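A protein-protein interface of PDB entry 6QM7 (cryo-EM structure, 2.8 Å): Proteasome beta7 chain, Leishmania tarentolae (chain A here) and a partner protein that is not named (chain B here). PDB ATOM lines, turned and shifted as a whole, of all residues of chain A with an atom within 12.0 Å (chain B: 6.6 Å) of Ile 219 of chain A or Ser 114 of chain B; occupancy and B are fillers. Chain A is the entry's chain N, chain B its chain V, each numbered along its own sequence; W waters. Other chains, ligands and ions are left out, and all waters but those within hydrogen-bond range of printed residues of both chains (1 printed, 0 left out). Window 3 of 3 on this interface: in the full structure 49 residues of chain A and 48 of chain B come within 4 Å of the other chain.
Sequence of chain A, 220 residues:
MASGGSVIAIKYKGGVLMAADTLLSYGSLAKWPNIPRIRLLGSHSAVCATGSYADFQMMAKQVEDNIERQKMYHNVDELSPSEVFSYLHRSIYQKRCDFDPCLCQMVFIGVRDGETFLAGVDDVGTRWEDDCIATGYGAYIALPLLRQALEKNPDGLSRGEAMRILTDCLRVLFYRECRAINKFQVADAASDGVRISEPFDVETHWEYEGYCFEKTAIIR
The backbone carbonyl oxygen (O) of Leu 91 of chain B is in hydrogen-bond range of the side-chain hydroxyl (OG) of Ser 114 of chain B, 3.0 Å away.
The backbone carbonyl oxygen (O) of Cys 97 of chain B lies within hydrogen-bond range of the backbone NH (N) of Thr 89 of chain B (2.8 Å).
Ile 218 of chain A touches Thr 89 of chain B (CG1 to OG1, 3.9 Å).
Ile 218 of chain A touches Gln 107 of chain B (CD1 to NE2, 3.9 Å).
Thr 89 of chain B touches Ile 219 of chain A (CG2 to CD1, 3.5 Å).
Lys 90 of chain B touches Ile 219 of chain A (O to CD1, 3.3 Å).
O of Ala 110 of chain B touches CD1 of Ile 219 of chain A (3.5 Å).
Glu 111 of chain B touches Ile 219 of chain A.
Ile 219 of chain A touches Ser 114 of chain B (CG2 to OG, 3.6 Å).
Cys 212 of chain A touches none of the printed residues of chain B.
Of the printed residues of chain B, Ile 218 of chain A touches Thr 89 and Gln 107.
Ile 219 of chain A touches just these residues of chain B: Thr 89 (3.5 Å), Lys 90 (3.3 Å), Ala 110 (3.5 Å), Glu 111 (3.8 Å) and Ser 114 (3.6 Å).
Thr 89 of chain B touches just these residues of chain A: Ile 218 and Ile 219.
Lys 90 of chain B touches just one residue of chain A: Ile 219.
Printed residues of chain A within 4 Å of Gln 107 of chain B: Ile 218.
Of chain A, only Ile 219 comes within 4 Å of Ala 110 of chain B.
No residue of chain A comes within 4 Å of Val 113 of chain B.
Ser 114 of chain B touches one residue of chain A.
No residue of chain A comes within 4 Å of Asn 115 of chain B.
No residue of chain A comes within 4 Å of Leu 117 of chain B.
The nearest printed residue of chain A that does not touch Gln 107 of chain B is Ile 219 of chain A (5.3 Å).
Hydrophobic or aromatic side chains of chain A that line the printed part of chain B: Ile 218 and Ile 219.
Of the 19 printed residues of chain B, 6 touch a printed residue of chain A.
Among the printed residues, 7 pairs touch across the chains.
Among the printed residues, no Asp or Glu carboxylate lies within 4 Å of a Lys or Arg side-chain nitrogen of the other chain.
Water W1 bridges the side-chain hydroxyl of Thr 89 of chain B (2.8 Å) and the backbone NH of Ile 218 of chain A (3.2 Å).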
ATOM      1  N   CYS A 212     -24.763 -17.153 -17.544  1.00  0.00           N
ATOM      2  CA  CYS A 212     -23.384 -16.639 -17.748  1.00  0.00           C
ATOM      3  C   CYS A 212     -23.111 -15.479 -16.773  1.00  0.00           C
ATOM      4  O   CYS A 212     -24.061 -14.817 -16.321  1.00  0.00           O
ATOM      5  CB  CYS A 212     -23.166 -16.195 -19.185  1.00  0.00           C
ATOM      6  SG  CYS A 212     -23.837 -14.543 -19.511  1.00  0.00           S
ATOM      7  N   PHE A 213     -21.842 -15.273 -16.447  1.00  0.00           N
ATOM      8  CA  PHE A 213     -21.363 -14.284 -15.453  1.00  0.00           C
ATOM      9  C   PHE A 213     -21.844 -12.881 -15.812  1.00  0.00           C
ATOM     10  O   PHE A 213     -22.208 -12.143 -14.898  1.00  0.00           O
ATOM     11  CB  PHE A 213     -19.834 -14.292 -15.412  1.00  0.00           C
ATOM     12  CG  PHE A 213     -19.237 -13.591 -14.225  1.00  0.00           C
ATOM     13  CD1 PHE A 213     -18.844 -14.313 -13.112  1.00  0.00           C
ATOM     14  CD2 PHE A 213     -19.064 -12.216 -14.229  1.00  0.00           C
ATOM     15  CE1 PHE A 213     -18.289 -13.668 -12.022  1.00  0.00           C
ATOM     16  CE2 PHE A 213     -18.516 -11.569 -13.129  1.00  0.00           C
ATOM     17  CZ  PHE A 213     -18.123 -12.297 -12.029  1.00  0.00           C
ATOM     18  N   GLU A 214     -21.795 -12.529 -17.102  1.00  0.00           N
ATOM     19  CA  GLU A 214     -22.053 -11.159 -17.616  1.00  0.00           C
ATOM     20  C   GLU A 214     -23.532 -10.802 -17.430  1.00  0.00           C
ATOM     21  O   GLU A 214     -23.793  -9.674 -16.993  1.00  0.00           O
ATOM     22  CB  GLU A 214     -21.639 -11.046 -19.081  1.00  0.00           C
ATOM     23  CG  GLU A 214     -21.440  -9.608 -19.531  1.00  0.00           C
ATOM     24  CD  GLU A 214     -21.260  -9.401 -21.032  1.00  0.00           C
ATOM     25  OE1 GLU A 214     -20.271  -9.928 -21.593  1.00  0.00           O
ATOM     26  OE2 GLU A 214     -22.110  -8.708 -21.644  1.00  0.00           O
ATOM     27  N   LYS A 215     -24.459 -11.711 -17.741  1.00  0.00           N
ATOM     28  CA  LYS A 215     -25.925 -11.458 -17.641  1.00  0.00           C
ATOM     29  C   LYS A 215     -26.336 -11.347 -16.174  1.00  0.00           C
ATOM     30  O   LYS A 215     -26.968 -10.331 -15.821  1.00  0.00           O
ATOM     31  CB  LYS A 215     -26.744 -12.558 -18.325  1.00  0.00           C
ATOM     32  CG  LYS A 215     -26.597 -12.614 -19.838  1.00  0.00           C
ATOM     33  CD  LYS A 215     -27.410 -11.570 -20.597  1.00  0.00           C
ATOM     34  CE  LYS A 215     -28.548 -12.170 -21.398  1.00  0.00           C
ATOM     35  NZ  LYS A 215     -28.068 -13.212 -22.339  1.00  0.00           N
ATOM     36  N   THR A 216     -25.974 -12.343 -15.362  1.00  0.00           N
ATOM     37  CA  THR A 216     -26.407 -12.495 -13.949  1.00  0.00           C
ATOM     38  C   THR A 216     -25.738 -11.466 -13.032  1.00  0.00           C
ATOM     39  O   THR A 216     -26.148 -11.383 -11.860  1.00  0.00           O
ATOM     40  CB  THR A 216     -26.114 -13.900 -13.411  1.00  0.00           C
ATOM     41  OG1 THR A 216     -24.732 -14.186 -13.617  1.00  0.00           O
ATOM     42  CG2 THR A 216     -26.964 -14.959 -14.076  1.00  0.00           C
ATOM     43  N   ALA A 217     -24.730 -10.747 -13.519  1.00  0.00           N
ATOM     44  CA  ALA A 217     -24.055  -9.653 -12.791  1.00  0.00           C
ATOM     45  C   ALA A 217     -25.082  -8.611 -12.343  1.00  0.00           C
ATOM     46  O   ALA A 217     -25.979  -8.295 -13.128  1.00  0.00           O
ATOM     47  CB  ALA A 217     -23.006  -9.036 -13.671  1.00  0.00           C
ATOM     48  N   ILE A 218     -24.937  -8.113 -11.120  1.00  0.00           N
ATOM     49  CA  ILE A 218     -25.789  -7.047 -10.522  1.00  0.00           C
ATOM     50  C   ILE A 218     -25.358  -5.697 -11.105  1.00  0.00           C
ATOM     51  O   ILE A 218     -26.219  -4.826 -11.219  1.00  0.00           O
ATOM     52  CB  ILE A 218     -25.676  -7.069  -8.978  1.00  0.00           C
ATOM     53  CG1 ILE A 218     -25.974  -8.454  -8.387  1.00  0.00           C
ATOM     54  CG2 ILE A 218     -26.545  -5.991  -8.334  1.00  0.00           C
ATOM     55  CD1 ILE A 218     -27.291  -9.051  -8.820  1.00  0.00           C
ATOM     56  N   ILE A 219     -24.071  -5.538 -11.444  1.00  0.00           N
ATOM     57  CA  ILE A 219     -23.429  -4.253 -11.865  1.00  0.00           C
ATOM     58  C   ILE A 219     -22.499  -4.525 -13.056  1.00  0.00           C
ATOM     59  O   ILE A 219     -22.676  -3.889 -14.106  1.00  0.00           O
ATOM     60  CB  ILE A 219     -22.683  -3.641 -10.660  1.00  0.00           C
ATOM     61  CG1 ILE A 219     -23.608  -3.446  -9.452  1.00  0.00           C
ATOM     62  CG2 ILE A 219     -21.976  -2.346 -11.031  1.00  0.00           C
ATOM     63  CD1 ILE A 219     -22.900  -3.052  -8.177  1.00  0.00           C
ATOM     64  N   THR B  89     -19.719  -9.229  -7.282  1.00  0.00           N
ATOM     65  CA  THR B  89     -20.406  -8.000  -7.716  1.00  0.00           C
ATOM     66  C   THR B  89     -19.354  -6.930  -7.926  1.00  0.00           C
ATOM     67  O   THR B  89     -18.683  -6.583  -6.946  1.00  0.00           O
ATOM     68  CB  THR B  89     -21.496  -7.626  -6.714  1.00  0.00           C
ATOM     69  OG1 THR B  89     -22.445  -8.691  -6.794  1.00  0.00           O
ATOM     70  CG2 THR B  89     -22.136  -6.285  -7.006  1.00  0.00           C
ATOM     71  N   LYS B  90     -19.250  -6.448  -9.162  1.00  0.00           N
ATOM     72  CA  LYS B  90     -18.302  -5.391  -9.597  1.00  0.00           C
ATOM     73  C   LYS B  90     -18.541  -4.150  -8.744  1.00  0.00           C
ATOM     74  O   LYS B  90     -19.700  -3.852  -8.479  1.00  0.00           O
ATOM     75  CB  LYS B  90     -18.525  -5.127 -11.085  1.00  0.00           C
ATOM     76  CG  LYS B  90     -17.602  -4.131 -11.752  1.00  0.00           C
ATOM     77  CD  LYS B  90     -18.084  -3.790 -13.150  1.00  0.00           C
ATOM     78  CE  LYS B  90     -17.662  -2.413 -13.632  1.00  0.00           C
ATOM     79  NZ  LYS B  90     -16.377  -2.459 -14.375  1.00  0.00           N
ATOM     80  N   LEU B  91     -17.483  -3.506  -8.267  1.00  0.00           N
ATOM     81  CA  LEU B  91     -17.560  -2.155  -7.667  1.00  0.00           C
ATOM     82  C   LEU B  91     -16.852  -1.183  -8.606  1.00  0.00           C
ATOM     83  O   LEU B  91     -17.459  -0.151  -8.947  1.00  0.00           O
ATOM     84  CB  LEU B  91     -16.935  -2.172  -6.270  1.00  0.00           C
ATOM     85  CG  LEU B  91     -17.576  -3.133  -5.270  1.00  0.00           C
ATOM     86  CD1 LEU B  91     -16.862  -3.076  -3.926  1.00  0.00           C
ATOM     87  CD2 LEU B  91     -19.054  -2.820  -5.086  1.00  0.00           C
ATOM     88  N   THR B  92     -15.617  -1.503  -8.987  1.00  0.00           N
ATOM     89  CA  THR B  92     -14.869  -0.823 -10.075  1.00  0.00           C
ATOM     90  C   THR B  92     -14.347  -1.888 -11.035  1.00  0.00           C
ATOM     91  O   THR B  92     -14.640  -3.071 -10.803  1.00  0.00           O
ATOM     92  CB  THR B  92     -13.744   0.077  -9.541  1.00  0.00           C
ATOM     93  OG1 THR B  92     -12.625  -0.705  -9.119  1.00  0.00           O
ATOM     94  CG2 THR B  92     -14.210   0.960  -8.407  1.00  0.00           C
ATOM     95  N   CYS B  97     -16.719  -7.218  -4.911  1.00  0.00           N
ATOM     96  CA  CYS B  97     -17.117  -7.735  -3.587  1.00  0.00           C
ATOM     97  C   CYS B  97     -17.792  -9.089  -3.780  1.00  0.00           C
ATOM     98  O   CYS B  97     -18.308  -9.344  -4.852  1.00  0.00           O
ATOM     99  CB  CYS B  97     -18.044  -6.763  -2.876  1.00  0.00           C
ATOM    100  SG  CYS B  97     -19.532  -6.399  -3.834  1.00  0.00           S
ATOM    101  N   GLN B 107     -26.911  -6.293  -2.372  1.00  0.00           N
ATOM    102  CA  GLN B 107     -27.116  -5.700  -3.713  1.00  0.00           C
ATOM    103  C   GLN B 107     -27.218  -4.189  -3.572  1.00  0.00           C
ATOM    104  O   GLN B 107     -26.533  -3.487  -4.319  1.00  0.00           O
ATOM    105  CB  GLN B 107     -28.388  -6.229  -4.363  1.00  0.00           C
ATOM    106  CG  GLN B 107     -28.208  -7.601  -5.000  1.00  0.00           C
ATOM    107  CD  GLN B 107     -29.465  -8.085  -5.673  1.00  0.00           C
ATOM    108  OE1 GLN B 107     -30.272  -7.299  -6.158  1.00  0.00           O
ATOM    109  NE2 GLN B 107     -29.642  -9.393  -5.709  1.00  0.00           N
ATOM    110  N   LEU B 109     -26.177  -2.202  -1.009  1.00  0.00           N
ATOM    111  CA  LEU B 109     -24.846  -1.696  -0.578  1.00  0.00           C
ATOM    112  C   LEU B 109     -23.882  -1.727  -1.763  1.00  0.00           C
ATOM    113  O   LEU B 109     -23.185  -0.732  -1.967  1.00  0.00           O
ATOM    114  CB  LEU B 109     -24.289  -2.548   0.565  1.00  0.00           C
ATOM    115  CG  LEU B 109     -25.012  -2.429   1.906  1.00  0.00           C
ATOM    116  CD1 LEU B 109     -24.465  -3.437   2.914  1.00  0.00           C
ATOM    117  CD2 LEU B 109     -24.906  -1.020   2.451  1.00  0.00           C
ATOM    118  N   ALA B 110     -23.823  -2.831  -2.499  1.00  0.00           N
ATOM    119  CA  ALA B 110     -22.858  -2.992  -3.605  1.00  0.00           C
ATOM    120  C   ALA B 110     -23.121  -1.919  -4.660  1.00  0.00           C
ATOM    121  O   ALA B 110     -22.157  -1.396  -5.210  1.00  0.00           O
ATOM    122  CB  ALA B 110     -22.930  -4.371  -4.195  1.00  0.00           C
ATOM    123  N   GLU B 111     -24.387  -1.605  -4.921  1.00  0.00           N
ATOM    124  CA  GLU B 111     -24.798  -0.597  -5.927  1.00  0.00           C
ATOM    125  C   GLU B 111     -24.488   0.794  -5.392  1.00  0.00           C
ATOM    126  O   GLU B 111     -24.065   1.637  -6.195  1.00  0.00           O
ATOM    127  CB  GLU B 111     -26.283  -0.723  -6.257  1.00  0.00           C
ATOM    128  CG  GLU B 111     -26.577  -1.844  -7.244  1.00  0.00           C
ATOM    129  CD  GLU B 111     -28.054  -2.194  -7.419  1.00  0.00           C
ATOM    130  OE1 GLU B 111     -28.706  -2.498  -6.393  1.00  0.00           O
ATOM    131  OE2 GLU B 111     -28.561  -2.144  -8.578  1.00  0.00           O
ATOM    132  N   ARG B 112     -24.730   1.024  -4.101  1.00  0.00           N
ATOM    133  CA  ARG B 112     -24.444   2.320  -3.434  1.00  0.00           C
ATOM    134  C   ARG B 112     -22.943   2.565  -3.497  1.00  0.00           C
ATOM    135  O   ARG B 112     -22.553   3.635  -3.952  1.00  0.00           O
ATOM    136  CB  ARG B 112     -24.929   2.319  -1.985  1.00  0.00           C
ATOM    137  CG  ARG B 112     -24.835   3.662  -1.269  1.00  0.00           C
ATOM    138  CD  ARG B 112     -25.751   4.743  -1.808  1.00  0.00           C
ATOM    139  NE  ARG B 112     -25.127   5.441  -2.932  1.00  0.00           N
ATOM    140  CZ  ARG B 112     -25.631   6.498  -3.576  1.00  0.00           C
ATOM    141  NH1 ARG B 112     -24.951   7.042  -4.578  1.00  0.00           N
ATOM    142  NH2 ARG B 112     -26.804   7.009  -3.222  1.00  0.00           N
ATOM    143  N   VAL B 113     -22.149   1.580  -3.088  1.00  0.00           N
ATOM    144  CA  VAL B 113     -20.670   1.692  -2.984  1.00  0.00           C
ATOM    145  C   VAL B 113     -20.085   1.811  -4.377  1.00  0.00           C
ATOM    146  O   VAL B 113     -19.123   2.584  -4.523  1.00  0.00           O
ATOM    147  CB  VAL B 113     -20.062   0.502  -2.233  1.00  0.00           C
ATOM    148  CG1 VAL B 113     -18.556   0.376  -2.435  1.00  0.00           C
ATOM    149  CG2 VAL B 113     -20.395   0.603  -0.756  1.00  0.00           C
ATOM    150  N   SER B 114     -20.602   1.055  -5.342  1.00  0.00           N
ATOM    151  CA  SER B 114     -20.113   1.069  -6.741  1.00  0.00           C
ATOM    152  C   SER B 114     -20.289   2.476  -7.301  1.00  0.00           C
ATOM    153  O   SER B 114     -19.361   2.972  -7.965  1.00  0.00           O
ATOM    154  CB  SER B 114     -20.812   0.050  -7.569  1.00  0.00           C
ATOM    155  OG  SER B 114     -20.440   0.137  -8.936  1.00  0.00           O
ATOM    156  N   ASN B 115     -21.421   3.100  -6.986  1.00  0.00           N
ATOM    157  CA  ASN B 115     -21.791   4.463  -7.431  1.00  0.00           C
ATOM    158  C   ASN B 115     -20.864   5.488  -6.783  1.00  0.00           C
ATOM    159  O   ASN B 115     -20.472   6.412  -7.493  1.00  0.00           O
ATOM    160  CB  ASN B 115     -23.252   4.776  -7.117  1.00  0.00           C
ATOM    161  CG  ASN B 115     -23.738   6.020  -7.825  1.00  0.00           C
ATOM    162  OD1 ASN B 115     -23.616   7.130  -7.297  1.00  0.00           O
ATOM    163  ND2 ASN B 115     -24.259   5.840  -9.031  1.00  0.00           N
ATOM    164  N   TYR B 116     -20.551   5.366  -5.493  1.00  0.00           N
ATOM    165  CA  TYR B 116     -19.631   6.300  -4.789  1.00  0.00           C
ATOM    166  C   TYR B 116     -18.227   6.164  -5.372  1.00  0.00           C
ATOM    167  O   TYR B 116     -17.622   7.182  -5.647  1.00  0.00           O
ATOM    168  CB  TYR B 116     -19.580   6.067  -3.277  1.00  0.00           C
ATOM    169  CG  TYR B 116     -20.792   6.476  -2.479  1.00  0.00           C
ATOM    170  CD1 TYR B 116     -21.599   7.537  -2.858  1.00  0.00           C
ATOM    171  CD2 TYR B 116     -21.101   5.831  -1.293  1.00  0.00           C
ATOM    172  CE1 TYR B 116     -22.705   7.916  -2.114  1.00  0.00           C
ATOM    173  CE2 TYR B 116     -22.203   6.197  -0.532  1.00  0.00           C
ATOM    174  CZ  TYR B 116     -23.013   7.244  -0.947  1.00  0.00           C
ATOM    175  OH  TYR B 116     -24.105   7.629  -0.223  1.00  0.00           O
ATOM    176  N   LEU B 117     -17.742   4.942  -5.546  1.00  0.00           N
ATOM    177  CA  LEU B 117     -16.413   4.642  -6.140  1.00  0.00           C
ATOM    178  C   LEU B 117     -16.324   5.184  -7.562  1.00  0.00           C
ATOM    179  O   LEU B 117     -15.219   5.538  -7.955  1.00  0.00           O
ATOM    180  CB  LEU B 117     -16.198   3.124  -6.179  1.00  0.00           C
ATOM    181  CG  LEU B 117     -15.342   2.495  -5.083  1.00  0.00           C
ATOM    182  CD1 LEU B 117     -15.233   3.364  -3.840  1.00  0.00           C
ATOM    183  CD2 LEU B 117     -15.891   1.116  -4.740  1.00  0.00           C
ATOM    184  N   GLY B 118     -17.412   5.137  -8.328  1.00  0.00           N
ATOM    185  CA  GLY B 118     -17.435   5.643  -9.712  1.00  0.00           C
ATOM    186  C   GLY B 118     -17.290   7.151  -9.740  1.00  0.00           C
ATOM    187  O   GLY B 118     -16.474   7.649 -10.538  1.00  0.00           O
ATOM    188  N   SER B 119     -18.054   7.840  -8.885  1.00  0.00           N
ATOM    189  CA  SER B 119     -17.999   9.307  -8.675  1.00  0.00           C
ATOM    190  C   SER B 119     -16.595   9.692  -8.217  1.00  0.00           C
ATOM    191  O   SER B 119     -16.050  10.691  -8.740  1.00  0.00           O
ATOM    192  CB  SER B 119     -19.019   9.774  -7.671  1.00  0.00           C
ATOM    193  OG  SER B 119     -20.283   9.176  -7.904  1.00  0.00           O
ATOM    194  N   LEU B 136     -15.256   2.297   2.429  1.00  0.00           N
ATOM    195  CA  LEU B 136     -16.641   2.740   2.113  1.00  0.00           C
ATOM    196  C   LEU B 136     -17.633   1.669   2.529  1.00  0.00           C
ATOM    197  O   LEU B 136     -18.648   2.005   3.138  1.00  0.00           O
ATOM    198  CB  LEU B 136     -16.817   2.980   0.618  1.00  0.00           C
ATOM    199  CG  LEU B 136     -16.551   4.393   0.140  1.00  0.00           C
ATOM    200  CD1 LEU B 136     -17.038   4.522  -1.280  1.00  0.00           C
ATOM    201  CD2 LEU B 136     -17.251   5.409   1.020  1.00  0.00           C
ATOM    202  N   PHE B 137     -17.360   0.436   2.131  1.00  0.00           N
ATOM    203  CA  PHE B 137     -18.239  -0.725   2.380  1.00  0.00           C
ATOM    204  C   PHE B 137     -18.386  -0.938   3.874  1.00  0.00           C
ATOM    205  O   PHE B 137     -19.475  -1.298   4.294  1.00  0.00           O
ATOM    206  CB  PHE B 137     -17.674  -1.986   1.744  1.00  0.00           C
ATOM    207  CG  PHE B 137     -18.666  -2.641   0.840  1.00  0.00           C
ATOM    208  CD1 PHE B 137     -19.857  -3.108   1.357  1.00  0.00           C
ATOM    209  CD2 PHE B 137     -18.426  -2.741  -0.515  1.00  0.00           C
ATOM    210  CE1 PHE B 137     -20.787  -3.716   0.535  1.00  0.00           C
ATOM    211  CE2 PHE B 137     -19.347  -3.360  -1.337  1.00  0.00           C
ATOM    212  CZ  PHE B 137     -20.526  -3.845  -0.814  1.00  0.00           C
HETATM  213  O   HOH W   1     -22.880  -9.761  -9.347  1.00  0.00           O
